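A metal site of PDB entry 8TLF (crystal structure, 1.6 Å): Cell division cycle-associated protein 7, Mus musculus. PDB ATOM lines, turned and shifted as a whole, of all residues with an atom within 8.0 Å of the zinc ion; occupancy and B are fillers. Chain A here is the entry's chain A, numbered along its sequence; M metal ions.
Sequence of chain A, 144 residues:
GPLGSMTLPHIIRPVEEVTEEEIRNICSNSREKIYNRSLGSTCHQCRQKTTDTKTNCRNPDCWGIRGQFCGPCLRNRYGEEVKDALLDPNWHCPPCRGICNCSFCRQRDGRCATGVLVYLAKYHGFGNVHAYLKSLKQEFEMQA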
ATOM      1  N   HIS A  44       5.088   5.939  -8.095  1.00  0.00           N
ATOM      2  CA  HIS A  44       5.464   6.951  -9.080  1.00  0.00           C
ATOM      3  C   HIS A  44       6.981   7.012  -9.262  1.00  0.00           C
ATOM      4  O   HIS A  44       7.454   7.267 -10.380  1.00  0.00           O
ATOM      5  CB  HIS A  44       4.940   8.324  -8.662  1.00  0.00           C
ATOM      6  CG  HIS A  44       5.433   9.448  -9.517  1.00  0.00           C
ATOM      7  ND1 HIS A  44       5.013   9.637 -10.808  1.00  0.00           N
ATOM      8  CD2 HIS A  44       6.333  10.424  -9.260  1.00  0.00           C
ATOM      9  CE1 HIS A  44       5.623  10.699 -11.314  1.00  0.00           C
ATOM     10  NE2 HIS A  44       6.427  11.194 -10.402  1.00  0.00           N
ATOM     11  N   GLN A  45       7.748   6.784  -8.195  1.00  0.00           N
ATOM     12  CA  GLN A  45       9.194   6.961  -8.267  1.00  0.00           C
ATOM     13  C   GLN A  45       9.855   5.842  -9.061  1.00  0.00           C
ATOM     14  O   GLN A  45      10.566   6.093 -10.036  1.00  0.00           O
ATOM     15  CB  GLN A  45       9.772   7.042  -6.847  1.00  0.00           C
ATOM     16  CG  GLN A  45      11.236   7.466  -6.796  1.00  0.00           C
ATOM     17  CD  GLN A  45      11.415   8.964  -6.921  1.00  0.00           C
ATOM     18  OE1 GLN A  45      10.488   9.733  -6.674  1.00  0.00           O
ATOM     19  NE2 GLN A  45      12.612   9.387  -7.303  1.00  0.00           N
ATOM     20  N   ARG A  47       8.213   3.196 -10.520  1.00  0.00           N
ATOM     21  CA  ARG A  47       7.344   2.736 -11.599  1.00  0.00           C
ATOM     22  C   ARG A  47       7.142   1.214 -11.582  1.00  0.00           C
ATOM     23  O   ARG A  47       6.970   0.582 -12.629  1.00  0.00           O
ATOM     24  CB  ARG A  47       7.873   3.192 -12.969  1.00  0.00           C
ATOM     25  CG  ARG A  47       8.045   4.714 -13.056  1.00  0.00           C
ATOM     26  CD  ARG A  47       8.380   5.187 -14.462  1.00  0.00           C
ATOM     27  NE  ARG A  47       9.776   4.955 -14.821  1.00  0.00           N
ATOM     28  CZ  ARG A  47      10.769   5.784 -14.547  1.00  0.00           C
ATOM     29  NH1 ARG A  47      10.561   6.906 -13.876  1.00  0.00           N
ATOM     30  NH2 ARG A  47      12.005   5.486 -14.950  1.00  0.00           N
ATOM     31  N   ARG A  66       0.161   9.829  -9.493  1.00  0.00           N
ATOM     32  CA  ARG A  66       1.419  10.529  -9.226  1.00  0.00           C
ATOM     33  C   ARG A  66       1.705  10.632  -7.732  1.00  0.00           C
ATOM     34  O   ARG A  66       2.863  10.823  -7.342  1.00  0.00           O
ATOM     35  CB  ARG A  66       1.390  11.914  -9.865  1.00  0.00           C
ATOM     36  CG  ARG A  66       0.322  12.840  -9.303  1.00  0.00           C
ATOM     37  CD  ARG A  66      -0.039  13.946 -10.285  1.00  0.00           C
ATOM     38  NE  ARG A  66       1.017  14.944 -10.434  1.00  0.00           N
ATOM     39  CZ  ARG A  66       1.066  16.081  -9.757  1.00  0.00           C
ATOM     40  NH1 ARG A  66       0.152  16.403  -8.865  1.00  0.00           N
ATOM     41  NH2 ARG A  66       2.061  16.932  -9.994  1.00  0.00           N
ATOM     42  N   PHE A  69       3.624   6.456  -3.614  1.00  0.00           N
ATOM     43  CA  PHE A  69       5.038   6.158  -3.414  1.00  0.00           C
ATOM     44  C   PHE A  69       5.185   4.972  -2.478  1.00  0.00           C
ATOM     45  O   PHE A  69       4.476   4.865  -1.475  1.00  0.00           O
ATOM     46  CB  PHE A  69       5.785   7.372  -2.845  1.00  0.00           C
ATOM     47  CG  PHE A  69       5.963   8.489  -3.834  1.00  0.00           C
ATOM     48  CD1 PHE A  69       4.935   9.373  -4.112  1.00  0.00           C
ATOM     49  CD2 PHE A  69       7.175   8.659  -4.490  1.00  0.00           C
ATOM     50  CE1 PHE A  69       5.103  10.402  -5.018  1.00  0.00           C
ATOM     51  CE2 PHE A  69       7.350   9.695  -5.394  1.00  0.00           C
ATOM     52  CZ  PHE A  69       6.315  10.552  -5.661  1.00  0.00           C
ATOM     53  N   TYR A  78      13.165  11.080  -0.345  1.00  0.00           N
ATOM     54  CA  TYR A  78      12.598  12.270   0.285  1.00  0.00           C
ATOM     55  C   TYR A  78      12.709  12.278   1.809  1.00  0.00           C
ATOM     56  O   TYR A  78      12.306  13.266   2.427  1.00  0.00           O
ATOM     57  CB  TYR A  78      11.129  12.429  -0.112  1.00  0.00           C
ATOM     58  CG  TYR A  78      10.929  12.405  -1.620  1.00  0.00           C
ATOM     59  CD1 TYR A  78      11.174  13.540  -2.380  1.00  0.00           C
ATOM     60  CD2 TYR A  78      10.515  11.249  -2.263  1.00  0.00           C
ATOM     61  CE1 TYR A  78      11.004  13.519  -3.752  1.00  0.00           C
ATOM     62  CE2 TYR A  78      10.346  11.228  -3.635  1.00  0.00           C
ATOM     63  CZ  TYR A  78      10.595  12.363  -4.372  1.00  0.00           C
ATOM     64  OH  TYR A  78      10.421  12.344  -5.734  1.00  0.00           O
ATOM     65  N   PRO A  94       5.234  14.580  -3.394  1.00  0.00           N
ATOM     66  CA  PRO A  94       6.326  15.418  -3.906  1.00  0.00           C
ATOM     67  C   PRO A  94       6.004  16.056  -5.248  1.00  0.00           C
ATOM     68  O   PRO A  94       6.397  17.211  -5.489  1.00  0.00           O
ATOM     69  CB  PRO A  94       7.505  14.428  -4.022  1.00  0.00           C
ATOM     70  CG  PRO A  94       7.220  13.422  -2.963  1.00  0.00           C
ATOM     71  CD  PRO A  94       5.722  13.281  -2.907  1.00  0.00           C
ATOM     72  N   PRO A  95       5.301  15.367  -6.168  1.00  0.00           N
ATOM     73  CA  PRO A  95       4.842  16.075  -7.370  1.00  0.00           C
ATOM     74  C   PRO A  95       3.963  17.276  -7.074  1.00  0.00           C
ATOM     75  O   PRO A  95       4.092  18.310  -7.732  1.00  0.00           O
ATOM     76  CB  PRO A  95       4.083  14.994  -8.149  1.00  0.00           C
ATOM     77  CG  PRO A  95       4.766  13.741  -7.777  1.00  0.00           C
ATOM     78  CD  PRO A  95       5.108  13.907  -6.320  1.00  0.00           C
ATOM     79  N   ILE A  99       8.737  18.925  -5.936  1.00  0.00           N
ATOM     80  CA  ILE A  99      10.070  18.559  -5.467  1.00  0.00           C
ATOM     81  C   ILE A  99      10.393  17.129  -5.871  1.00  0.00           C
ATOM     82  O   ILE A  99      11.360  16.543  -5.379  1.00  0.00           O
ATOM     83  CB  ILE A  99      10.195  18.744  -3.946  1.00  0.00           C
ATOM     84  CG1 ILE A  99       9.161  17.874  -3.215  1.00  0.00           C
ATOM     85  CG2 ILE A  99      10.034  20.202  -3.559  1.00  0.00           C
ATOM     86  CD1 ILE A  99       9.255  17.941  -1.707  1.00  0.00           C
ATOM     87  N   CYS A 100       9.599  16.554  -6.769  1.00  0.00           N
ATOM     88  CA  CYS A 100       9.832  15.192  -7.201  1.00  0.00           C
ATOM     89  C   CYS A 100      11.154  15.099  -7.953  1.00  0.00           C
ATOM     90  O   CYS A 100      11.459  15.948  -8.809  1.00  0.00           O
ATOM     91  CB  CYS A 100       8.691  14.694  -8.080  1.00  0.00           C
ATOM     92  SG  CYS A 100       8.796  12.935  -8.503  1.00  0.00           S
ATOM     93  N   ASN A 101      11.951  14.085  -7.634  1.00  0.00           N
ATOM     94  CA  ASN A 101      13.269  13.901  -8.233  1.00  0.00           C
ATOM     95  C   ASN A 101      13.361  12.590  -9.002  1.00  0.00           C
ATOM     96  O   ASN A 101      14.458  12.037  -9.173  1.00  0.00           O
ATOM     97  CB  ASN A 101      14.366  13.985  -7.160  1.00  0.00           C
ATOM     98  CG  ASN A 101      14.107  13.061  -5.988  1.00  0.00           C
ATOM     99  OD1 ASN A 101      13.667  11.926  -6.158  1.00  0.00           O
ATOM    100  ND2 ASN A 101      14.391  13.543  -4.783  1.00  0.00           N
ATOM    101  N   CYS A 102      12.221  12.072  -9.457  1.00  0.00           N
ATOM    102  CA  CYS A 102      12.235  10.882 -10.298  1.00  0.00           C
ATOM    103  C   CYS A 102      12.831  11.221 -11.657  1.00  0.00           C
ATOM    104  O   CYS A 102      12.984  12.395 -12.033  1.00  0.00           O
ATOM    105  CB  CYS A 102      10.822  10.310 -10.441  1.00  0.00           C
ATOM    106  SG  CYS A 102       9.739  11.176 -11.617  1.00  0.00           S
ATOM    107  N   SER A 103      13.171  10.177 -12.420  1.00  0.00           N
ATOM    108  CA  SER A 103      13.863  10.365 -13.684  1.00  0.00           C
ATOM    109  C   SER A 103      13.040  11.169 -14.678  1.00  0.00           C
ATOM    110  O   SER A 103      13.599  11.817 -15.569  1.00  0.00           O
ATOM    111  CB  SER A 103      14.233   9.010 -14.286  1.00  0.00           C
ATOM    112  OG  SER A 103      13.074   8.260 -14.590  1.00  0.00           O
ATOM    113  N   PHE A 104      11.714  11.150 -14.557  1.00  0.00           N
ATOM    114  CA  PHE A 104      10.900  11.905 -15.497  1.00  0.00           C
ATOM    115  C   PHE A 104      10.739  13.358 -15.064  1.00  0.00           C
ATOM    116  O   PHE A 104      10.889  14.274 -15.877  1.00  0.00           O
ATOM    117  CB  PHE A 104       9.537  11.225 -15.671  1.00  0.00           C
ATOM    118  CG  PHE A 104       8.581  11.998 -16.523  1.00  0.00           C
ATOM    119  CD1 PHE A 104       8.662  11.957 -17.898  1.00  0.00           C
ATOM    120  CD2 PHE A 104       7.584  12.766 -15.932  1.00  0.00           C
ATOM    121  CE1 PHE A 104       7.769  12.674 -18.682  1.00  0.00           C
ATOM    122  CE2 PHE A 104       6.696  13.476 -16.712  1.00  0.00           C
ATOM    123  CZ  PHE A 104       6.785  13.441 -18.085  1.00  0.00           C
ATOM    124  N   CYS A 105      10.465  13.593 -13.767  1.00  0.00           N
ATOM    125  CA  CYS A 105      10.153  14.933 -13.292  1.00  0.00           C
ATOM    126  C   CYS A 105      11.383  15.840 -13.217  1.00  0.00           C
ATOM    127  O   CYS A 105      11.252  17.048 -13.417  1.00  0.00           O
ATOM    128  CB  CYS A 105       9.478  14.855 -11.922  1.00  0.00           C
ATOM    129  SG  CYS A 105       7.810  14.159 -11.969  1.00  0.00           S
ATOM    130  N   ARG A 106      12.562  15.286 -12.929  1.00  0.00           N
ATOM    131  CA  ARG A 106      13.745  16.131 -12.802  1.00  0.00           C
ATOM    132  C   ARG A 106      14.328  16.530 -14.152  1.00  0.00           C
ATOM    133  O   ARG A 106      15.281  17.327 -14.181  1.00  0.00           O
ATOM    134  CB  ARG A 106      14.815  15.421 -11.960  1.00  0.00           C
ATOM    135  CG  ARG A 106      15.507  14.247 -12.634  1.00  0.00           C
ATOM    136  CD  ARG A 106      16.622  13.705 -11.746  1.00  0.00           C
ATOM    137  NE  ARG A 106      17.295  12.552 -12.342  1.00  0.00           N
ATOM    138  CZ  ARG A 106      17.038  11.297 -12.016  1.00  0.00           C
ATOM    139  NH1 ARG A 106      16.121  10.984 -11.119  1.00  0.00           N
ATOM    140  NH2 ARG A 106      17.725  10.320 -12.616  1.00  0.00           N
HETATM  141 ZN    ZN M   1       8.085  12.380 -10.583  1.00  0.00          ZN
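SG of Cys 102 sits close to N of Phe 104, 3.5 Å away. NE2 of Gln 45 lies close to N of Cys 102 (3.5 Å). SG of Cys 100 lies close to OH of Tyr 78 (3.3 Å).
Four residues have an atom within 4 Å of the zinc ion: His 44, Cys 100, Cys 102 and Cys 105.
The zinc ion is bound by a ring nitrogen (NE2) of His 44 (2.0 Å), the side-chain sulfur (SG) of Cys 100 (2.3 Å), the side-chain sulfur (SG) of Cys 105 (2.3 Å) and the side-chain sulfur (SG) of Cys 102 (2.3 Å). The zinc ion has four donor atoms within binding distance.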
